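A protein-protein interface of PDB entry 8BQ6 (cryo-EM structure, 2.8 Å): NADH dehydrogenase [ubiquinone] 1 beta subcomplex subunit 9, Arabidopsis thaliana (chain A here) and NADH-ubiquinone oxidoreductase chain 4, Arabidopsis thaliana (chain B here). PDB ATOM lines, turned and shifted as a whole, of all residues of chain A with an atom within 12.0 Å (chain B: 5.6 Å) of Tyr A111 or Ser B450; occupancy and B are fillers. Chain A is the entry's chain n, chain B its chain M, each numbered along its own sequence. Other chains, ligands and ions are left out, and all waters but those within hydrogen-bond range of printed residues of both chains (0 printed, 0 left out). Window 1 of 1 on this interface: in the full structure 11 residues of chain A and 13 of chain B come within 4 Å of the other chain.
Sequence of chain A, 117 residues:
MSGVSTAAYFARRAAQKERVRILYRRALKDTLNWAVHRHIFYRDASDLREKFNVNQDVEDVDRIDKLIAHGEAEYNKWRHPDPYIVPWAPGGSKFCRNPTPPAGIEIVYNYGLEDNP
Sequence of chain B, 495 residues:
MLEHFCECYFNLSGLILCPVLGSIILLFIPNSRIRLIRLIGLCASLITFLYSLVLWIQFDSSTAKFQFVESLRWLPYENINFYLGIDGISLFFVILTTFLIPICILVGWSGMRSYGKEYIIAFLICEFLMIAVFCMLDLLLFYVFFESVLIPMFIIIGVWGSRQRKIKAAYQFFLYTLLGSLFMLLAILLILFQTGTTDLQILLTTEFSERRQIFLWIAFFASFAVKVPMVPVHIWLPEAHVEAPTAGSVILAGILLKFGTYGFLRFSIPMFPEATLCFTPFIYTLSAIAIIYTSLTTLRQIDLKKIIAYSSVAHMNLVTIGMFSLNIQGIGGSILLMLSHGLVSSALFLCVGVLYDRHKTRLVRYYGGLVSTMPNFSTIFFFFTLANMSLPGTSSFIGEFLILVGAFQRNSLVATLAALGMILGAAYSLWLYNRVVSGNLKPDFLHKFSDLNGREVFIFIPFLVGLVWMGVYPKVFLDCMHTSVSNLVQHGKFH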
ATOM      1  N   GLY A 104     -24.187  14.301   4.811  1.00  0.00           N
ATOM      2  CA  GLY A 104     -23.341  15.377   4.337  1.00  0.00           C
ATOM      3  C   GLY A 104     -23.989  16.295   3.331  1.00  0.00           C
ATOM      4  O   GLY A 104     -23.290  17.111   2.718  1.00  0.00           O
ATOM      5  N   ILE A 105     -25.299  16.188   3.139  1.00  0.00           N
ATOM      6  CA  ILE A 105     -26.037  16.991   2.174  1.00  0.00           C
ATOM      7  C   ILE A 105     -26.568  18.218   2.903  1.00  0.00           C
ATOM      8  O   ILE A 105     -27.183  18.096   3.969  1.00  0.00           O
ATOM      9  CB  ILE A 105     -27.187  16.191   1.543  1.00  0.00           C
ATOM     10  CG1 ILE A 105     -26.682  14.912   0.861  1.00  0.00           C
ATOM     11  CG2 ILE A 105     -27.940  17.047   0.548  1.00  0.00           C
ATOM     12  CD1 ILE A 105     -25.519  15.101  -0.073  1.00  0.00           C
ATOM     13  N   GLU A 106     -26.262  19.396   2.353  1.00  0.00           N
ATOM     14  CA  GLU A 106     -26.746  20.665   2.948  1.00  0.00           C
ATOM     15  C   GLU A 106     -27.622  21.400   1.938  1.00  0.00           C
ATOM     16  O   GLU A 106     -27.331  21.317   0.741  1.00  0.00           O
ATOM     17  CB  GLU A 106     -25.573  21.548   3.374  1.00  0.00           C
ATOM     18  CG  GLU A 106     -24.731  20.963   4.492  1.00  0.00           C
ATOM     19  CD  GLU A 106     -23.300  20.672   4.078  1.00  0.00           C
ATOM     20  OE1 GLU A 106     -22.380  21.006   4.848  1.00  0.00           O
ATOM     21  OE2 GLU A 106     -23.111  20.123   2.983  1.00  0.00           O
ATOM     22  N   ILE A 107     -28.646  22.097   2.410  1.00  0.00           N
ATOM     23  CA  ILE A 107     -29.592  22.827   1.576  1.00  0.00           C
ATOM     24  C   ILE A 107     -29.469  24.306   1.904  1.00  0.00           C
ATOM     25  O   ILE A 107     -29.616  24.706   3.065  1.00  0.00           O
ATOM     26  CB  ILE A 107     -31.033  22.333   1.795  1.00  0.00           C
ATOM     27  CG1 ILE A 107     -31.176  20.870   1.373  1.00  0.00           C
ATOM     28  CG2 ILE A 107     -32.005  23.182   1.016  1.00  0.00           C
ATOM     29  CD1 ILE A 107     -30.672  20.574  -0.016  1.00  0.00           C
ATOM     30  N   VAL A 108     -29.166  25.096   0.871  1.00  0.00           N
ATOM     31  CA  VAL A 108     -28.962  26.560   1.045  1.00  0.00           C
ATOM     32  C   VAL A 108     -30.259  27.317   0.774  1.00  0.00           C
ATOM     33  O   VAL A 108     -30.891  27.058  -0.264  1.00  0.00           O
ATOM     34  CB  VAL A 108     -27.827  27.061   0.128  1.00  0.00           C
ATOM     35  CG1 VAL A 108     -27.511  28.533   0.332  1.00  0.00           C
ATOM     36  CG2 VAL A 108     -26.573  26.212   0.255  1.00  0.00           C
ATOM     37  N   TYR A 109     -30.654  28.196   1.688  1.00  0.00           N
ATOM     38  CA  TYR A 109     -31.817  29.054   1.541  1.00  0.00           C
ATOM     39  C   TYR A 109     -31.378  30.452   1.132  1.00  0.00           C
ATOM     40  O   TYR A 109     -30.250  30.870   1.409  1.00  0.00           O
ATOM     41  CB  TYR A 109     -32.619  29.134   2.841  1.00  0.00           C
ATOM     42  CG  TYR A 109     -33.348  27.864   3.190  1.00  0.00           C
ATOM     43  CD1 TYR A 109     -33.738  26.975   2.202  1.00  0.00           C
ATOM     44  CD2 TYR A 109     -33.655  27.558   4.506  1.00  0.00           C
ATOM     45  CE1 TYR A 109     -34.405  25.815   2.514  1.00  0.00           C
ATOM     46  CE2 TYR A 109     -34.328  26.398   4.827  1.00  0.00           C
ATOM     47  CZ  TYR A 109     -34.699  25.531   3.826  1.00  0.00           C
ATOM     48  OH  TYR A 109     -35.370  24.373   4.139  1.00  0.00           O
ATOM     49  N   ASN A 110     -32.287  31.172   0.476  1.00  0.00           N
ATOM     50  CA  ASN A 110     -32.042  32.548   0.035  1.00  0.00           C
ATOM     51  C   ASN A 110     -30.801  32.642  -0.852  1.00  0.00           C
ATOM     52  O   ASN A 110     -29.901  33.448  -0.610  1.00  0.00           O
ATOM     53  CB  ASN A 110     -31.939  33.501   1.230  1.00  0.00           C
ATOM     54  CG  ASN A 110     -32.978  33.210   2.298  1.00  0.00           C
ATOM     55  OD1 ASN A 110     -34.179  33.308   2.052  1.00  0.00           O
ATOM     56  ND2 ASN A 110     -32.521  32.846   3.489  1.00  0.00           N
ATOM     57  N   TYR A 111     -30.758  31.816  -1.894  1.00  0.00           N
ATOM     58  CA  TYR A 111     -29.686  31.877  -2.874  1.00  0.00           C
ATOM     59  C   TYR A 111     -30.049  32.835  -4.004  1.00  0.00           C
ATOM     60  O   TYR A 111     -31.211  32.948  -4.400  1.00  0.00           O
ATOM     61  CB  TYR A 111     -29.402  30.489  -3.455  1.00  0.00           C
ATOM     62  CG  TYR A 111     -28.314  30.499  -4.500  1.00  0.00           C
ATOM     63  CD1 TYR A 111     -26.978  30.516  -4.135  1.00  0.00           C
ATOM     64  CD2 TYR A 111     -28.624  30.535  -5.852  1.00  0.00           C
ATOM     65  CE1 TYR A 111     -25.982  30.540  -5.084  1.00  0.00           C
ATOM     66  CE2 TYR A 111     -27.636  30.565  -6.807  1.00  0.00           C
ATOM     67  CZ  TYR A 111     -26.316  30.567  -6.418  1.00  0.00           C
ATOM     68  OH  TYR A 111     -25.327  30.595  -7.371  1.00  0.00           O
ATOM     69  N   GLY A 112     -29.035  33.525  -4.524  1.00  0.00           N
ATOM     70  CA  GLY A 112     -29.199  34.368  -5.695  1.00  0.00           C
ATOM     71  C   GLY A 112     -30.049  35.607  -5.507  1.00  0.00           C
ATOM     72  O   GLY A 112     -30.762  36.005  -6.434  1.00  0.00           O
ATOM     73  N   LEU A 113     -29.977  36.241  -4.341  1.00  0.00           N
ATOM     74  CA  LEU A 113     -30.733  37.460  -4.089  1.00  0.00           C
ATOM     75  C   LEU A 113     -30.082  38.647  -4.797  1.00  0.00           C
ATOM     76  O   LEU A 113     -28.879  38.649  -5.072  1.00  0.00           O
ATOM     77  CB  LEU A 113     -30.821  37.715  -2.583  1.00  0.00           C
ATOM     78  CG  LEU A 113     -31.352  36.556  -1.730  1.00  0.00           C
ATOM     79  CD1 LEU A 113     -31.507  36.966  -0.279  1.00  0.00           C
ATOM     80  CD2 LEU A 113     -32.680  36.059  -2.274  1.00  0.00           C
ATOM     81  N   GLU A 114     -30.892  39.669  -5.098  1.00  0.00           N
ATOM     82  CA  GLU A 114     -30.374  40.814  -5.845  1.00  0.00           C
ATOM     83  C   GLU A 114     -29.315  41.577  -5.061  1.00  0.00           C
ATOM     84  O   GLU A 114     -28.415  42.176  -5.659  1.00  0.00           O
ATOM     85  CB  GLU A 114     -31.506  41.760  -6.238  1.00  0.00           C
ATOM     86  CG  GLU A 114     -32.256  42.343  -5.069  1.00  0.00           C
ATOM     87  CD  GLU A 114     -33.154  43.477  -5.488  1.00  0.00           C
ATOM     88  OE1 GLU A 114     -34.178  43.702  -4.817  1.00  0.00           O
ATOM     89  OE2 GLU A 114     -32.829  44.152  -6.485  1.00  0.00           O
ATOM     90  N   ASP A 115     -29.402  41.569  -3.737  1.00  0.00           N
ATOM     91  CA  ASP A 115     -28.413  42.235  -2.903  1.00  0.00           C
ATOM     92  C   ASP A 115     -27.157  41.389  -2.759  1.00  0.00           C
ATOM     93  O   ASP A 115     -26.106  41.891  -2.365  1.00  0.00           O
ATOM     94  CB  ASP A 115     -29.005  42.545  -1.531  1.00  0.00           C
ATOM     95  CG  ASP A 115     -29.959  43.716  -1.567  1.00  0.00           C
ATOM     96  OD1 ASP A 115     -29.925  44.471  -2.560  1.00  0.00           O
ATOM     97  OD2 ASP A 115     -30.750  43.872  -0.614  1.00  0.00           O
ATOM     98  N   ASP B 357     -24.368  28.281 -12.505  1.00  0.00           N
ATOM     99  CA  ASP B 357     -24.170  29.401 -11.591  1.00  0.00           C
ATOM    100  C   ASP B 357     -23.907  28.926 -10.171  1.00  0.00           C
ATOM    101  O   ASP B 357     -23.171  29.582  -9.424  1.00  0.00           O
ATOM    102  CB  ASP B 357     -25.385  30.325 -11.611  1.00  0.00           C
ATOM    103  CG  ASP B 357     -25.593  30.982 -12.954  1.00  0.00           C
ATOM    104  OD1 ASP B 357     -26.539  31.787 -13.079  1.00  0.00           O
ATOM    105  OD2 ASP B 357     -24.811  30.693 -13.884  1.00  0.00           O
ATOM    106  N   ARG B 358     -24.498  27.800  -9.778  1.00  0.00           N
ATOM    107  CA  ARG B 358     -24.307  27.267  -8.436  1.00  0.00           C
ATOM    108  C   ARG B 358     -23.028  26.451  -8.310  1.00  0.00           C
ATOM    109  O   ARG B 358     -22.230  26.682  -7.396  1.00  0.00           O
ATOM    110  CB  ARG B 358     -25.501  26.404  -8.027  1.00  0.00           C
ATOM    111  CG  ARG B 358     -26.799  27.150  -7.892  1.00  0.00           C
ATOM    112  CD  ARG B 358     -27.958  26.227  -8.168  1.00  0.00           C
ATOM    113  NE  ARG B 358     -29.215  26.773  -7.676  1.00  0.00           N
ATOM    114  CZ  ARG B 358     -29.877  27.760  -8.258  1.00  0.00           C
ATOM    115  NH1 ARG B 358     -29.431  28.336  -9.363  1.00  0.00           N
ATOM    116  NH2 ARG B 358     -31.018  28.180  -7.721  1.00  0.00           N
ATOM    117  N   HIS B 359     -22.879  25.439  -9.173  1.00  0.00           N
ATOM    118  CA  HIS B 359     -21.772  24.454  -9.013  1.00  0.00           C
ATOM    119  C   HIS B 359     -20.563  24.685  -9.924  1.00  0.00           C
ATOM    120  O   HIS B 359     -19.546  24.025  -9.669  1.00  0.00           O
ATOM    121  CB  HIS B 359     -22.360  23.055  -9.206  1.00  0.00           C
ATOM    122  CG  HIS B 359     -23.667  22.850  -8.514  1.00  0.00           C
ATOM    123  ND1 HIS B 359     -23.807  22.970  -7.146  1.00  0.00           N
ATOM    124  CD2 HIS B 359     -24.891  22.538  -8.990  1.00  0.00           C
ATOM    125  CE1 HIS B 359     -25.057  22.732  -6.809  1.00  0.00           C
ATOM    126  NE2 HIS B 359     -25.742  22.469  -7.922  1.00  0.00           N
ATOM    127  N   THR B 373     -32.776  16.827  -4.435  1.00  0.00           N
ATOM    128  CA  THR B 373     -32.447  18.105  -3.820  1.00  0.00           C
ATOM    129  C   THR B 373     -33.074  19.296  -4.521  1.00  0.00           C
ATOM    130  O   THR B 373     -33.279  20.331  -3.880  1.00  0.00           O
ATOM    131  CB  THR B 373     -30.926  18.309  -3.777  1.00  0.00           C
ATOM    132  OG1 THR B 373     -30.373  18.096  -5.081  1.00  0.00           O
ATOM    133  CG2 THR B 373     -30.298  17.326  -2.813  1.00  0.00           C
ATOM    134  N   MET B 374     -33.369  19.183  -5.812  1.00  0.00           N
ATOM    135  CA  MET B 374     -33.972  20.267  -6.588  1.00  0.00           C
ATOM    136  C   MET B 374     -35.150  19.733  -7.395  1.00  0.00           C
ATOM    137  O   MET B 374     -35.121  19.721  -8.628  1.00  0.00           O
ATOM    138  CB  MET B 374     -32.930  20.908  -7.505  1.00  0.00           C
ATOM    139  CG  MET B 374     -31.527  20.938  -6.929  1.00  0.00           C
ATOM    140  SD  MET B 374     -30.254  21.292  -8.153  1.00  0.00           S
ATOM    141  CE  MET B 374     -30.776  22.897  -8.739  1.00  0.00           C
ATOM    142  N   LYS B 448     -23.777  20.496  -1.444  1.00  0.00           N
ATOM    143  CA  LYS B 448     -24.553  21.685  -1.007  1.00  0.00           C
ATOM    144  C   LYS B 448     -25.480  22.078  -2.157  1.00  0.00           C
ATOM    145  O   LYS B 448     -24.957  22.275  -3.269  1.00  0.00           O
ATOM    146  CB  LYS B 448     -23.583  22.799  -0.600  1.00  0.00           C
ATOM    147  CG  LYS B 448     -24.220  24.037   0.008  1.00  0.00           C
ATOM    148  CD  LYS B 448     -23.326  25.253  -0.054  1.00  0.00           C
ATOM    149  CE  LYS B 448     -21.962  25.014   0.558  1.00  0.00           C
ATOM    150  NZ  LYS B 448     -21.160  26.258   0.613  1.00  0.00           N
ATOM    151  N   PHE B 449     -26.788  22.213  -1.907  1.00  0.00           N
ATOM    152  CA  PHE B 449     -27.735  22.424  -3.035  1.00  0.00           C
ATOM    153  C   PHE B 449     -28.831  23.454  -2.762  1.00  0.00           C
ATOM    154  O   PHE B 449     -29.313  23.556  -1.637  1.00  0.00           O
ATOM    155  CB  PHE B 449     -28.447  21.111  -3.378  1.00  0.00           C
ATOM    156  CG  PHE B 449     -27.552  19.976  -3.794  1.00  0.00           C
ATOM    157  CD1 PHE B 449     -27.147  19.018  -2.878  1.00  0.00           C
ATOM    158  CD2 PHE B 449     -27.114  19.863  -5.103  1.00  0.00           C
ATOM    159  CE1 PHE B 449     -26.327  17.972  -3.263  1.00  0.00           C
ATOM    160  CE2 PHE B 449     -26.288  18.819  -5.484  1.00  0.00           C
ATOM    161  CZ  PHE B 449     -25.900  17.875  -4.565  1.00  0.00           C
ATOM    162  N   SER B 450     -29.240  24.168  -3.806  1.00  0.00           N
ATOM    163  CA  SER B 450     -30.334  25.120  -3.706  1.00  0.00           C
ATOM    164  C   SER B 450     -31.217  24.953  -4.928  1.00  0.00           C
ATOM    165  O   SER B 450     -30.720  24.967  -6.059  1.00  0.00           O
ATOM    166  CB  SER B 450     -29.820  26.559  -3.616  1.00  0.00           C
ATOM    167  OG  SER B 450     -30.854  27.441  -3.228  1.00  0.00           O
ATOM    168  N   ASP B 451     -32.517  24.793  -4.700  1.00  0.00           N
ATOM    169  CA  ASP B 451     -33.475  24.768  -5.790  1.00  0.00           C
ATOM    170  C   ASP B 451     -33.673  26.179  -6.335  1.00  0.00           C
ATOM    171  O   ASP B 451     -33.047  27.145  -5.891  1.00  0.00           O
ATOM    172  CB  ASP B 451     -34.797  24.170  -5.319  1.00  0.00           C
ATOM    173  CG  ASP B 451     -35.500  23.389  -6.406  1.00  0.00           C
ATOM    174  OD1 ASP B 451     -35.193  23.612  -7.593  1.00  0.00           O
ATOM    175  OD2 ASP B 451     -36.353  22.545  -6.074  1.00  0.00           O
ATOM    176  N   LEU B 452     -34.569  26.299  -7.309  1.00  0.00           N
ATOM    177  CA  LEU B 452     -34.800  27.584  -7.947  1.00  0.00           C
ATOM    178  C   LEU B 452     -35.347  28.593  -6.953  1.00  0.00           C
ATOM    179  O   LEU B 452     -36.098  28.248  -6.036  1.00  0.00           O
ATOM    180  CB  LEU B 452     -35.770  27.437  -9.114  1.00  0.00           C
ATOM    181  CG  LEU B 452     -35.507  26.277 -10.065  1.00  0.00           C
ATOM    182  CD1 LEU B 452     -36.715  26.064 -10.939  1.00  0.00           C
ATOM    183  CD2 LEU B 452     -34.277  26.561 -10.902  1.00  0.00           C
ATOM    184  N   ASN B 453     -34.958  29.849  -7.134  1.00  0.00           N
ATOM    185  CA  ASN B 453     -35.517  30.923  -6.337  1.00  0.00           C
ATOM    186  C   ASN B 453     -36.653  31.597  -7.102  1.00  0.00           C
ATOM    187  O   ASN B 453     -37.046  31.171  -8.192  1.00  0.00           O
ATOM    188  CB  ASN B 453     -34.428  31.918  -5.938  1.00  0.00           C
ATOM    189  CG  ASN B 453     -33.672  32.482  -7.128  1.00  0.00           C
ATOM    190  OD1 ASN B 453     -34.258  33.045  -8.051  1.00  0.00           O
ATOM    191  ND2 ASN B 453     -32.355  32.348  -7.099  1.00  0.00           N
ATOM    192  N   GLU B 456     -35.844  32.757 -10.744  1.00  0.00           N
ATOM    193  CA  GLU B 456     -35.667  31.709 -11.744  1.00  0.00           C
ATOM    194  C   GLU B 456     -36.993  31.056 -12.115  1.00  0.00           C
ATOM    195  O   GLU B 456     -37.209  30.707 -13.280  1.00  0.00           O
ATOM    196  CB  GLU B 456     -34.682  30.658 -11.240  1.00  0.00           C
ATOM    197  CG  GLU B 456     -33.232  31.059 -11.378  1.00  0.00           C
ATOM    198  CD  GLU B 456     -32.369  30.472 -10.286  1.00  0.00           C
ATOM    199  OE1 GLU B 456     -31.237  30.038 -10.581  1.00  0.00           O
ATOM    200  OE2 GLU B 456     -32.819  30.446  -9.125  1.00  0.00           O
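Among the printed residues, merely in contact across the chains: Val A108 with Lys B448 (3.2 Å), Glu A106 with Lys B448 (3.3 Å), Ile A107 with Phe B449 (3.3 Å), Tyr A111 with Ser B450 (3.4 Å) and Tyr A111 with Arg B358 (3.6 Å).
O of Ser B450 is in hydrogen-bond range of NE of Arg B358 (2.9 Å). NH2 of Arg B358 sits at hydrogen-bond distance from O of Asp B451 (2.9 Å). The side-chain carboxylate (OE1) of Glu B456 lies within salt-bridge range of the guanidinium group (NH1) of Arg B358, at 2.8 Å. The side-chain amide nitrogen (ND2) of Asn B453 lies within hydrogen-bond range of the side-chain carboxylate (OE2) of Glu B456 (2.8 Å).
The backbone carbonyl oxygen (O) of Asp B357 is in hydrogen-bond range of the side-chain hydroxyl (OH) of Tyr A111. N of Phe B449 lies within hydrogen-bond range of O of Glu A106 (2.8 Å). The backbone carbonyl oxygen (O) of Phe B449 is in hydrogen-bond range of the backbone NH (N) of Val A108, at 2.9 Å. The side-chain hydroxyl (OG) of Ser B450 is in hydrogen-bond range of the backbone carbonyl oxygen (O) of Val A108. The side-chain amide nitrogen of Asn B453 lies within hydrogen-bond range of the backbone carbonyl oxygen of Tyr A111 (3.0 Å).
Hydrophobic or aromatic side chains of chain A within 4 Å of the printed part of chain B: Ile A107, Val A108 and Tyr A111. Of the 12 printed residues of chain B, 6 touch a printed residue of chain A. Printed residues of chain B that touch a printed residue of chain A: Asp B357, Arg B358, Lys B448, Phe B449, Ser B450 and Asn B453. Among the printed residues, 10 pairs touch across the chains.
Gly A104 touches none of the printed residues of chain B. Of the printed residues of chain B, Glu A106 touches Lys B448 (3.3 Å) and Phe B449 (2.8 Å). Printed residues of chain B within 4 Å of Ile A107: Phe B449. Printed residues of chain B within 4 Å of Val A108: Lys B448, Phe B449 and Ser B450. Of chain B, only Asp B357, Arg B358, Ser B450 and Asn B453 come within 4 Å of Tyr A111. Asp B357 touches just one residue of chain A: Tyr A111 (3.1 Å). Printed residues of chain A within 4 Å of Lys B448: Glu A106 (3.3 Å) and Val A108 (3.2 Å). Phe B449 touches just these residues of chain A: Glu A106 (2.8 Å), Ile A107 (3.3 Å) and Val A108 (2.9 Å). Of chain A, only Val A108 and Tyr A111 come within 4 Å of Ser B450. Of the printed residues of chain A, Asn B453 touches Tyr A111 (3.0 Å).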
